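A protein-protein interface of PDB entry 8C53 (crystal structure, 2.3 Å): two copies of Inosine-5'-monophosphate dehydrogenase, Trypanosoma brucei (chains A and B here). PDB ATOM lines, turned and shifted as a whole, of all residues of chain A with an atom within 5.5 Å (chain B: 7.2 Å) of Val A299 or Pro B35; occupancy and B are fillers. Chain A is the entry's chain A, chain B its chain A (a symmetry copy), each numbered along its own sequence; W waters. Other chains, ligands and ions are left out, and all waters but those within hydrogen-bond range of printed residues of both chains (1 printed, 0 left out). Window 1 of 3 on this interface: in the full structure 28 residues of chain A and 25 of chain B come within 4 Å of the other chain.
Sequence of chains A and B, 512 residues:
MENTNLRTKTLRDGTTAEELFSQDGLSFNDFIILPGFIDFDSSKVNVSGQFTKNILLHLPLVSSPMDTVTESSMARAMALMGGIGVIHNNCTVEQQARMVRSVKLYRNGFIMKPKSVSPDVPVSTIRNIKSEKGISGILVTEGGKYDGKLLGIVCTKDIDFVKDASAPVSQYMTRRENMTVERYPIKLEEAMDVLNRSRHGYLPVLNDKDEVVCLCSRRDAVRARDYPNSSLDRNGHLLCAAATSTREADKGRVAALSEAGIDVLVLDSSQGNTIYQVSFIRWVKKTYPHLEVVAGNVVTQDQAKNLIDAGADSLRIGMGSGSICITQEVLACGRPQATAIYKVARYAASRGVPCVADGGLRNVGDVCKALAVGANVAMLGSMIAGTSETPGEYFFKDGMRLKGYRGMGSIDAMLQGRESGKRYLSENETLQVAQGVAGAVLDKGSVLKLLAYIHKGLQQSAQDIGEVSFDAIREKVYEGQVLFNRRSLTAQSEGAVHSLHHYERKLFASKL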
ATOM      1  N   GLN A 271       1.292  30.760 -22.527  1.00  0.00           N
ATOM      2  CA  GLN A 271       2.075  29.516 -22.547  1.00  0.00           C
ATOM      3  C   GLN A 271       1.062  28.382 -22.625  1.00  0.00           C
ATOM      4  O   GLN A 271       0.540  27.941 -21.603  1.00  0.00           O
ATOM      5  CB  GLN A 271       2.959  29.395 -21.322  1.00  0.00           C
ATOM      6  CG  GLN A 271       4.300  28.766 -21.597  1.00  0.00           C
ATOM      7  CD  GLN A 271       4.233  27.254 -21.620  1.00  0.00           C
ATOM      8  OE1 GLN A 271       3.594  26.656 -22.495  1.00  0.00           O
ATOM      9  NE2 GLN A 271       4.897  26.623 -20.658  1.00  0.00           N
ATOM     10  N   ASN A 297      -0.445  29.915 -26.942  1.00  0.00           N
ATOM     11  CA  ASN A 297       0.729  30.128 -27.781  1.00  0.00           C
ATOM     12  C   ASN A 297       1.883  29.193 -27.449  1.00  0.00           C
ATOM     13  O   ASN A 297       2.045  28.778 -26.307  1.00  0.00           O
ATOM     14  CB  ASN A 297       1.226  31.583 -27.628  1.00  0.00           C
ATOM     15  CG  ASN A 297       0.423  32.570 -28.439  1.00  0.00           C
ATOM     16  OD1 ASN A 297      -0.803  32.512 -28.472  1.00  0.00           O
ATOM     17  ND2 ASN A 297       1.116  33.485 -29.111  1.00  0.00           N
ATOM     18  N   VAL A 298       2.696  28.883 -28.459  1.00  0.00           N
ATOM     19  CA  VAL A 298       3.879  28.056 -28.283  1.00  0.00           C
ATOM     20  C   VAL A 298       5.037  28.697 -29.035  1.00  0.00           C
ATOM     21  O   VAL A 298       4.846  29.546 -29.911  1.00  0.00           O
ATOM     22  CB  VAL A 298       3.663  26.608 -28.784  1.00  0.00           C
ATOM     23  CG1 VAL A 298       2.458  25.992 -28.125  1.00  0.00           C
ATOM     24  CG2 VAL A 298       3.501  26.600 -30.292  1.00  0.00           C
ATOM     25  N   VAL A 299       6.253  28.295 -28.667  1.00  0.00           N
ATOM     26  CA  VAL A 299       7.442  28.744 -29.379  1.00  0.00           C
ATOM     27  C   VAL A 299       8.421  27.603 -29.642  1.00  0.00           C
ATOM     28  O   VAL A 299       9.440  27.807 -30.308  1.00  0.00           O
ATOM     29  CB  VAL A 299       8.128  29.891 -28.617  1.00  0.00           C
ATOM     30  CG1 VAL A 299       7.307  31.177 -28.726  1.00  0.00           C
ATOM     31  CG2 VAL A 299       8.314  29.517 -27.158  1.00  0.00           C
ATOM     32  N   THR A 300       8.146  26.405 -29.115  1.00  0.00           N
ATOM     33  CA  THR A 300       9.044  25.273 -29.340  1.00  0.00           C
ATOM     34  C   THR A 300       8.303  24.070 -29.913  1.00  0.00           C
ATOM     35  O   THR A 300       7.086  23.928 -29.782  1.00  0.00           O
ATOM     36  CB  THR A 300       9.758  24.799 -28.064  1.00  0.00           C
ATOM     37  OG1 THR A 300       8.818  24.070 -27.254  1.00  0.00           O
ATOM     38  CG2 THR A 300      10.307  25.976 -27.289  1.00  0.00           C
ATOM     39  N   GLN A 301       9.074  23.178 -30.531  1.00  0.00           N
ATOM     40  CA  GLN A 301       8.497  21.978 -31.120  1.00  0.00           C
ATOM     41  C   GLN A 301       7.922  21.032 -30.065  1.00  0.00           C
ATOM     42  O   GLN A 301       6.945  20.327 -30.343  1.00  0.00           O
ATOM     43  CB  GLN A 301       9.548  21.262 -31.964  1.00  0.00           C
ATOM     44  CG  GLN A 301      10.039  22.092 -33.129  1.00  0.00           C
ATOM     45  CD  GLN A 301      11.099  21.376 -33.966  1.00  0.00           C
ATOM     46  OE1 GLN A 301      11.688  20.383 -33.531  1.00  0.00           O
ATOM     47  NE2 GLN A 301      11.345  21.883 -35.177  1.00  0.00           N
ATOM     48  N   GLN A 303       6.323  21.835 -27.218  1.00  0.00           N
ATOM     49  CA  GLN A 303       4.977  22.340 -26.962  1.00  0.00           C
ATOM     50  C   GLN A 303       4.053  21.977 -28.108  1.00  0.00           C
ATOM     51  O   GLN A 303       2.930  21.495 -27.906  1.00  0.00           O
ATOM     52  CB  GLN A 303       5.003  23.856 -26.783  1.00  0.00           C
ATOM     53  CG  GLN A 303       5.871  24.387 -25.670  1.00  0.00           C
ATOM     54  CD  GLN A 303       6.000  25.906 -25.745  1.00  0.00           C
ATOM     55  OE1 GLN A 303       6.518  26.447 -26.715  1.00  0.00           O
ATOM     56  NE2 GLN A 303       5.523  26.595 -24.720  1.00  0.00           N
ATOM     57  N   ILE A 317       1.937  30.959 -32.876  1.00  0.00           N
ATOM     58  CA  ILE A 317       3.345  30.979 -32.514  1.00  0.00           C
ATOM     59  C   ILE A 317       3.716  32.361 -31.999  1.00  0.00           C
ATOM     60  O   ILE A 317       3.502  33.358 -32.692  1.00  0.00           O
ATOM     61  CB  ILE A 317       4.248  30.619 -33.705  1.00  0.00           C
ATOM     62  CG1 ILE A 317       3.963  29.221 -34.201  1.00  0.00           C
ATOM     63  CG2 ILE A 317       5.711  30.779 -33.299  1.00  0.00           C
ATOM     64  CD1 ILE A 317       4.659  28.884 -35.499  1.00  0.00           C
ATOM     65  N   GLY A 318       4.314  32.411 -30.811  1.00  0.00           N
ATOM     66  CA  GLY A 318       4.829  33.651 -30.274  1.00  0.00           C
ATOM     67  C   GLY A 318       4.816  33.715 -28.760  1.00  0.00           C
ATOM     68  O   GLY A 318       3.819  33.377 -28.115  1.00  0.00           O
ATOM     69  N   MET A 319       5.932  34.155 -28.184  1.00  0.00           N
ATOM     70  CA  MET A 319       6.025  34.374 -26.744  1.00  0.00           C
ATOM     71  C   MET A 319       7.198  35.320 -26.535  1.00  0.00           C
ATOM     72  O   MET A 319       8.350  34.922 -26.734  1.00  0.00           O
ATOM     73  CB  MET A 319       6.222  33.067 -25.994  1.00  0.00           C
ATOM     74  CG  MET A 319       6.541  33.244 -24.508  1.00  0.00           C
ATOM     75  SD  MET A 319       6.928  31.689 -23.670  1.00  0.00           S
ATOM     76  CE  MET A 319       5.745  31.692 -22.343  1.00  0.00           C
ATOM     77  N   CYS A 333      11.359  33.959 -19.930  1.00  0.00           N
ATOM     78  CA  CYS A 333      10.968  32.808 -20.731  1.00  0.00           C
ATOM     79  C   CYS A 333      10.280  33.263 -22.006  1.00  0.00           C
ATOM     80  O   CYS A 333       9.342  34.065 -21.966  1.00  0.00           O
ATOM     81  CB  CYS A 333      10.057  31.893 -19.908  1.00  0.00           C
ATOM     82  SG  CYS A 333       9.363  30.521 -20.803  1.00  0.00           S
ATOM     83  N   GLY A 334      10.763  32.750 -23.134  1.00  0.00           N
ATOM     84  CA  GLY A 334      10.259  33.153 -24.433  1.00  0.00           C
ATOM     85  C   GLY A 334      11.196  32.673 -25.522  1.00  0.00           C
ATOM     86  O   GLY A 334      11.968  31.742 -25.313  1.00  0.00           O
ATOM     87  N   ARG A 335      11.123  33.324 -26.690  1.00  0.00           N
ATOM     88  CA  ARG A 335      11.995  32.944 -27.789  1.00  0.00           C
ATOM     89  C   ARG A 335      11.976  33.945 -28.936  1.00  0.00           C
ATOM     90  O   ARG A 335      10.917  34.501 -29.261  1.00  0.00           O
ATOM     91  CB  ARG A 335      11.594  31.556 -28.322  1.00  0.00           C
ATOM     92  CG  ARG A 335      12.587  30.962 -29.326  1.00  0.00           C
ATOM     93  CD  ARG A 335      12.171  29.584 -29.779  1.00  0.00           C
ATOM     94  NE  ARG A 335      13.320  28.783 -30.192  1.00  0.00           N
ATOM     95  CZ  ARG A 335      13.230  27.540 -30.642  1.00  0.00           C
ATOM     96  NH1 ARG A 335      12.058  26.929 -30.749  1.00  0.00           N
ATOM     97  NH2 ARG A 335      14.339  26.889 -30.977  1.00  0.00           N
ATOM     98  N   GLN A 337      11.399  35.508 -32.392  1.00  0.00           N
ATOM     99  CA  GLN A 337      10.171  35.129 -33.081  1.00  0.00           C
ATOM    100  C   GLN A 337      10.448  34.467 -34.427  1.00  0.00           C
ATOM    101  O   GLN A 337       9.697  33.578 -34.847  1.00  0.00           O
ATOM    102  CB  GLN A 337       9.282  36.362 -33.256  1.00  0.00           C
ATOM    103  CG  GLN A 337       7.954  36.080 -33.968  1.00  0.00           C
ATOM    104  CD  GLN A 337       7.032  35.194 -33.155  1.00  0.00           C
ATOM    105  OE1 GLN A 337       7.441  34.594 -32.160  1.00  0.00           O
ATOM    106  NE2 GLN A 337       5.771  35.117 -33.569  1.00  0.00           N
ATOM    107  N   ALA A 340      11.438  30.931 -33.667  1.00  0.00           N
ATOM    108  CA  ALA A 340      10.275  30.199 -33.174  1.00  0.00           C
ATOM    109  C   ALA A 340       9.358  29.822 -34.332  1.00  0.00           C
ATOM    110  O   ALA A 340       8.894  28.674 -34.438  1.00  0.00           O
ATOM    111  CB  ALA A 340       9.518  31.045 -32.149  1.00  0.00           C
ATOM    112  N   LYS A 343      11.018  26.974 -36.577  1.00  0.00           N
ATOM    113  CA  LYS A 343      11.070  25.654 -35.954  1.00  0.00           C
ATOM    114  C   LYS A 343       9.671  25.064 -35.785  1.00  0.00           C
ATOM    115  O   LYS A 343       9.399  23.930 -36.204  1.00  0.00           O
ATOM    116  CB  LYS A 343      11.782  25.759 -34.598  1.00  0.00           C
ATOM    117  CG  LYS A 343      13.210  26.296 -34.681  1.00  0.00           C
ATOM    118  CD  LYS A 343      14.191  25.201 -35.164  1.00  0.00           C
ATOM    119  CE  LYS A 343      15.631  25.532 -34.760  1.00  0.00           C
ATOM    120  NZ  LYS A 343      16.605  24.497 -35.216  1.00  0.00           N
ATOM    121  N   VAL A 344       8.768  25.820 -35.166  1.00  0.00           N
ATOM    122  CA  VAL A 344       7.449  25.270 -34.892  1.00  0.00           C
ATOM    123  C   VAL A 344       6.711  24.992 -36.193  1.00  0.00           C
ATOM    124  O   VAL A 344       6.084  23.944 -36.350  1.00  0.00           O
ATOM    125  CB  VAL A 344       6.656  26.207 -33.975  1.00  0.00           C
ATOM    126  CG1 VAL A 344       5.215  25.698 -33.826  1.00  0.00           C
ATOM    127  CG2 VAL A 344       7.347  26.327 -32.610  1.00  0.00           C
ATOM    128  N   LYS B   9      10.948  16.141 -22.695  1.00  0.00           N
ATOM    129  CA  LYS B   9      11.198  16.542 -24.069  1.00  0.00           C
ATOM    130  C   LYS B   9      12.017  15.451 -24.742  1.00  0.00           C
ATOM    131  O   LYS B   9      13.075  15.064 -24.232  1.00  0.00           O
ATOM    132  CB  LYS B   9      11.934  17.879 -24.137  1.00  0.00           C
ATOM    133  CG  LYS B   9      11.322  19.031 -23.310  1.00  0.00           C
ATOM    134  CD  LYS B   9      12.143  20.306 -23.511  1.00  0.00           C
ATOM    135  CE  LYS B   9      11.605  21.499 -22.745  1.00  0.00           C
ATOM    136  NZ  LYS B   9      11.400  21.209 -21.288  1.00  0.00           N
ATOM    137  N   ASP B  13      13.920  20.719 -28.803  1.00  0.00           N
ATOM    138  CA  ASP B  13      14.095  21.852 -29.707  1.00  0.00           C
ATOM    139  C   ASP B  13      14.575  23.035 -28.878  1.00  0.00           C
ATOM    140  O   ASP B  13      13.784  23.795 -28.325  1.00  0.00           O
ATOM    141  CB  ASP B  13      12.797  22.164 -30.434  1.00  0.00           C
ATOM    142  CG  ASP B  13      12.805  23.535 -31.060  1.00  0.00           C
ATOM    143  OD1 ASP B  13      13.909  24.034 -31.355  1.00  0.00           O
ATOM    144  OD2 ASP B  13      11.705  24.103 -31.262  1.00  0.00           O
ATOM    145  N   ILE B  32      17.690  33.546 -23.505  1.00  0.00           N
ATOM    146  CA  ILE B  32      16.368  33.401 -22.915  1.00  0.00           C
ATOM    147  C   ILE B  32      16.142  31.916 -22.662  1.00  0.00           C
ATOM    148  O   ILE B  32      16.777  31.056 -23.273  1.00  0.00           O
ATOM    149  CB  ILE B  32      15.261  33.995 -23.817  1.00  0.00           C
ATOM    150  CG1 ILE B  32      14.095  34.483 -22.954  1.00  0.00           C
ATOM    151  CG2 ILE B  32      14.780  32.974 -24.832  1.00  0.00           C
ATOM    152  CD1 ILE B  32      13.015  35.205 -23.732  1.00  0.00           C
ATOM    153  N   ILE B  33      15.245  31.624 -21.726  1.00  0.00           N
ATOM    154  CA  ILE B  33      14.920  30.259 -21.338  1.00  0.00           C
ATOM    155  C   ILE B  33      13.639  29.838 -22.044  1.00  0.00           C
ATOM    156  O   ILE B  33      12.647  30.575 -22.042  1.00  0.00           O
ATOM    157  CB  ILE B  33      14.764  30.134 -19.815  1.00  0.00           C
ATOM    158  CG1 ILE B  33      16.009  30.658 -19.116  1.00  0.00           C
ATOM    159  CG2 ILE B  33      14.492  28.684 -19.443  1.00  0.00           C
ATOM    160  CD1 ILE B  33      15.858  30.739 -17.603  1.00  0.00           C
ATOM    161  N   LEU B  34      13.655  28.662 -22.635  1.00  0.00           N
ATOM    162  CA  LEU B  34      12.502  28.197 -23.382  1.00  0.00           C
ATOM    163  C   LEU B  34      11.460  27.619 -22.430  1.00  0.00           C
ATOM    164  O   LEU B  34      11.807  27.103 -21.367  1.00  0.00           O
ATOM    165  CB  LEU B  34      12.921  27.155 -24.396  1.00  0.00           C
ATOM    166  CG  LEU B  34      13.833  27.634 -25.523  1.00  0.00           C
ATOM    167  CD1 LEU B  34      14.145  26.474 -26.471  1.00  0.00           C
ATOM    168  CD2 LEU B  34      13.206  28.778 -26.294  1.00  0.00           C
ATOM    169  N   PRO B  35      10.176  27.728 -22.776  1.00  0.00           N
ATOM    170  CA  PRO B  35       9.130  27.180 -21.914  1.00  0.00           C
ATOM    171  C   PRO B  35       9.033  25.667 -22.006  1.00  0.00           C
ATOM    172  O   PRO B  35       9.443  25.043 -22.983  1.00  0.00           O
ATOM    173  CB  PRO B  35       7.855  27.850 -22.439  1.00  0.00           C
ATOM    174  CG  PRO B  35       8.160  28.194 -23.844  1.00  0.00           C
ATOM    175  CD  PRO B  35       9.618  28.529 -23.882  1.00  0.00           C
ATOM    176  N   GLY B  36       8.460  25.087 -20.954  1.00  0.00           N
ATOM    177  CA  GLY B  36       8.218  23.665 -20.901  1.00  0.00           C
ATOM    178  C   GLY B  36       6.748  23.318 -20.817  1.00  0.00           C
ATOM    179  O   GLY B  36       5.947  23.804 -21.620  1.00  0.00           O
ATOM    180  N   PHE B  37       6.387  22.476 -19.846  1.00  0.00           N
ATOM    181  CA  PHE B  37       5.032  21.969 -19.688  1.00  0.00           C
ATOM    182  C   PHE B  37       4.504  22.311 -18.307  1.00  0.00           C
ATOM    183  O   PHE B  37       5.210  22.147 -17.312  1.00  0.00           O
ATOM    184  CB  PHE B  37       4.998  20.451 -19.888  1.00  0.00           C
ATOM    185  CG  PHE B  37       3.655  19.845 -19.654  1.00  0.00           C
ATOM    186  CD1 PHE B  37       2.676  19.908 -20.633  1.00  0.00           C
ATOM    187  CD2 PHE B  37       3.359  19.230 -18.458  1.00  0.00           C
ATOM    188  CE1 PHE B  37       1.430  19.353 -20.416  1.00  0.00           C
ATOM    189  CE2 PHE B  37       2.112  18.678 -18.237  1.00  0.00           C
ATOM    190  CZ  PHE B  37       1.152  18.740 -19.213  1.00  0.00           C
ATOM    191  N   ILE B  38       3.243  22.736 -18.241  1.00  0.00           N
ATOM    192  CA  ILE B  38       2.644  23.260 -17.019  1.00  0.00           C
ATOM    193  C   ILE B  38       1.493  22.357 -16.593  1.00  0.00           C
ATOM    194  O   ILE B  38       0.574  22.096 -17.382  1.00  0.00           O
ATOM    195  CB  ILE B  38       2.136  24.703 -17.207  1.00  0.00           C
ATOM    196  CG1 ILE B  38       3.282  25.641 -17.571  1.00  0.00           C
ATOM    197  CG2 ILE B  38       1.445  25.183 -15.941  1.00  0.00           C
ATOM    198  CD1 ILE B  38       2.827  26.921 -18.219  1.00  0.00           C
ATOM    199  N   GLN B 463       6.948  28.482 -13.251  1.00  0.00           N
ATOM    200  CA  GLN B 463       5.769  27.871 -13.852  1.00  0.00           C
ATOM    201  C   GLN B 463       5.889  27.857 -15.367  1.00  0.00           C
ATOM    202  O   GLN B 463       5.731  26.815 -16.009  1.00  0.00           O
ATOM    203  CB  GLN B 463       4.502  28.609 -13.430  1.00  0.00           C
ATOM    204  CG  GLN B 463       3.237  27.848 -13.768  1.00  0.00           C
ATOM    205  CD  GLN B 463       2.013  28.736 -13.854  1.00  0.00           C
ATOM    206  OE1 GLN B 463       2.118  29.960 -13.894  1.00  0.00           O
ATOM    207  NE2 GLN B 463       0.840  28.117 -13.886  1.00  0.00           N
ATOM    208  N   ASP B 464       6.200  29.012 -15.957  1.00  0.00           N
ATOM    209  CA  ASP B 464       6.337  29.058 -17.412  1.00  0.00           C
ATOM    210  C   ASP B 464       7.420  28.083 -17.885  1.00  0.00           C
ATOM    211  O   ASP B 464       7.278  27.428 -18.927  1.00  0.00           O
ATOM    212  CB  ASP B 464       6.642  30.477 -17.877  1.00  0.00           C
ATOM    213  CG  ASP B 464       5.375  31.263 -18.232  1.00  0.00           C
ATOM    214  OD1 ASP B 464       5.492  32.454 -18.609  1.00  0.00           O
ATOM    215  OD2 ASP B 464       4.262  30.701 -18.141  1.00  0.00           O
ATOM    216  N   ILE B 465       8.510  27.963 -17.122  1.00  0.00           N
ATOM    217  CA  ILE B 465       9.560  27.018 -17.492  1.00  0.00           C
ATOM    218  C   ILE B 465       9.064  25.587 -17.379  1.00  0.00           C
ATOM    219  O   ILE B 465       9.568  24.691 -18.072  1.00  0.00           O
ATOM    220  CB  ILE B 465      10.811  27.236 -16.628  1.00  0.00           C
ATOM    221  CG1 ILE B 465      11.522  28.517 -17.046  1.00  0.00           C
ATOM    222  CG2 ILE B 465      11.757  26.051 -16.756  1.00  0.00           C
ATOM    223  CD1 ILE B 465      12.489  29.031 -16.025  1.00  0.00           C
ATOM    224  N   GLY B 466       8.088  25.338 -16.513  1.00  0.00           N
ATOM    225  CA  GLY B 466       7.451  24.042 -16.431  1.00  0.00           C
ATOM    226  C   GLY B 466       7.948  23.119 -15.343  1.00  0.00           C
ATOM    227  O   GLY B 466       7.752  21.912 -15.452  1.00  0.00           O
ATOM    228  N   GLN B 481      17.143  18.956 -20.098  1.00  0.00           N
ATOM    229  CA  GLN B 481      15.696  18.975 -20.266  1.00  0.00           C
ATOM    230  C   GLN B 481      15.102  20.374 -20.135  1.00  0.00           C
ATOM    231  O   GLN B 481      13.947  20.587 -20.541  1.00  0.00           O
ATOM    232  CB  GLN B 481      15.028  18.054 -19.242  1.00  0.00           C
ATOM    233  CG  GLN B 481      15.088  16.578 -19.617  1.00  0.00           C
ATOM    234  CD  GLN B 481      14.223  16.241 -20.799  1.00  0.00           C
ATOM    235  OE1 GLN B 481      13.026  16.497 -20.795  1.00  0.00           O
ATOM    236  NE2 GLN B 481      14.822  15.659 -21.820  1.00  0.00           N
ATOM    237  N   LEU B 483      15.862  24.045 -21.622  1.00  0.00           N
ATOM    238  CA  LEU B 483      16.624  24.473 -22.781  1.00  0.00           C
ATOM    239  C   LEU B 483      16.565  25.985 -22.919  1.00  0.00           C
ATOM    240  O   LEU B 483      15.710  26.648 -22.344  1.00  0.00           O
ATOM    241  CB  LEU B 483      16.101  23.800 -24.052  1.00  0.00           C
ATOM    242  CG  LEU B 483      16.137  22.272 -24.000  1.00  0.00           C
ATOM    243  CD1 LEU B 483      15.544  21.627 -25.245  1.00  0.00           C
ATOM    244  CD2 LEU B 483      17.579  21.806 -23.803  1.00  0.00           C
ATOM    245  N   ASN B 485      17.795  29.606 -25.562  1.00  0.00           N
ATOM    246  CA  ASN B 485      18.126  30.136 -26.870  1.00  0.00           C
ATOM    247  C   ASN B 485      19.023  31.345 -26.673  1.00  0.00           C
ATOM    248  O   ASN B 485      18.679  32.261 -25.927  1.00  0.00           O
ATOM    249  CB  ASN B 485      16.883  30.521 -27.657  1.00  0.00           C
ATOM    250  CG  ASN B 485      16.632  29.599 -28.824  1.00  0.00           C
ATOM    251  OD1 ASN B 485      16.924  28.389 -28.759  1.00  0.00           O
ATOM    252  ND2 ASN B 485      16.080  30.150 -29.898  1.00  0.00           N
HETATM  253  O   HOH W   1       9.021  22.731 -24.520  1.00  0.00           O
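The backbone carbonyl oxygen (O) of Gly B36 sits at hydrogen-bond distance from the side-chain amide nitrogen (NE2) of Gln A271 (3.2 Å). O of Asp B464 lies within hydrogen-bond range of NE2 of Gln A271, 3.1 Å away. The backbone NH (N) of Gln A301 lies within hydrogen-bond range of the side-chain carboxylate (OD2) of Asp B13. The side-chain sulfur (SG) of Cys A333 sits close to the backbone carbonyl oxygen (O) of Ile B33. N of Gly A334 is in hydrogen-bond range of O of Ile B33 (3.1 Å). The guanidinium group (NH1) of Arg A335 lies within salt-bridge range of the side-chain carboxylate (OD2) of Asp B13 (2.9 Å). ND2 of Asn B485 lies close to NE of Arg A335 (3.1 Å). The backbone nitrogen (N) of Pro B35 sits close to the side-chain sulfur (SG) of Cys A333 (3.5 Å).
The side-chain amide oxygen (OE1) of Gln A271 is in hydrogen-bond range of the side-chain amide nitrogen (NE2) of Gln A303, at 2.9 Å. O of Val A299 sits at hydrogen-bond distance from NH1 of Arg A335, 2.8 Å away. The backbone NH of Thr A300 is in hydrogen-bond range of the side-chain amide oxygen of Gln A303 (2.9 Å). NE2 of Gln A301 sits at hydrogen-bond distance from O of Lys A343, 3.0 Å away. The backbone carbonyl oxygen (O) of Met A319 sits at hydrogen-bond distance from the backbone NH (N) of Arg A335, at 3.2 Å. The backbone NH (N) of Asn B485 sits at hydrogen-bond distance from the backbone carbonyl oxygen (O) of Ile B32.
Among the printed residues, merely in contact across the chains: Gly A334 with Ile B32, Gln A303 with Pro B35, Gln A271 with Ile B38, Gly A334 with Leu B34, Thr A300 with Asp B13, Val A299 with Pro B35, Gln A271 with Pro B35, Met A319 with Pro B35, Arg A335 with Leu B34, Lys A343 with Asp B13, Cys A333 with Ile B32, Met A319 with Asp B464, Cys A333 with Leu B34, Thr A300 with Leu B34, Arg A335 with Ile B32 and Cys A333 with Asp B464.
Of the printed residues of chain B, Val A299 touches Pro B35. Of the printed residues of chain B, Met A319 touches Pro B35 (3.7 Å) and Asp B464 (3.8 Å). Of the printed residues of chain B, Cys A333 touches Ile B32 (3.8 Å), Ile B33 (3.1 Å), Leu B34 (3.9 Å), Pro B35 (3.5 Å) and Asp B464 (3.996 Å). Printed residues of chain B within 4 Å of Gly A334: Ile B32, Ile B33 and Leu B34. Gln A337 touches none of the printed residues of chain B. Of the printed residues of chain A, Ile B38 touches Gln A271. Of the printed residues of chain A, Asp B464 touches Gln A271 (3.1 Å), Met A319 (3.8 Å) and Cys A333 (3.996 Å). Gln B481 touches none of the printed residues of chain A. The nearest residue of chain B that does not touch Val A299 is Asp B13 (4.4 Å). The nearest residue of chain A that does not touch Pro B35 is Gly A334 (4.2 Å).
Of the 16 printed residues of chain B, 9 touch a printed residue of chain A. Along chain B the printed residues that touch a printed residue of chain A span positions 13 to 485. Of the 17 printed residues of chain A, 10 touch a printed residue of chain B. Printed residues of chain A that touch a printed residue of chain B: Gln A271, Val A299, Thr A300, Gln A301, Gln A303, Met A319, Cys A333, Gly A334, Arg A335 and Lys A343. Among the printed residues, 24 pairs touch across the chains. Among the printed residues, Asp or Glu carboxylates within 4 Å of a Lys or Arg side-chain nitrogen of the other chain: Arg A335 with Asp B13.
No position is printed for both chains.
Water W1 lies within hydrogen-bond range of O of Pro B35 (2.8 Å) and OG1 of Thr A300 (3.1 Å).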
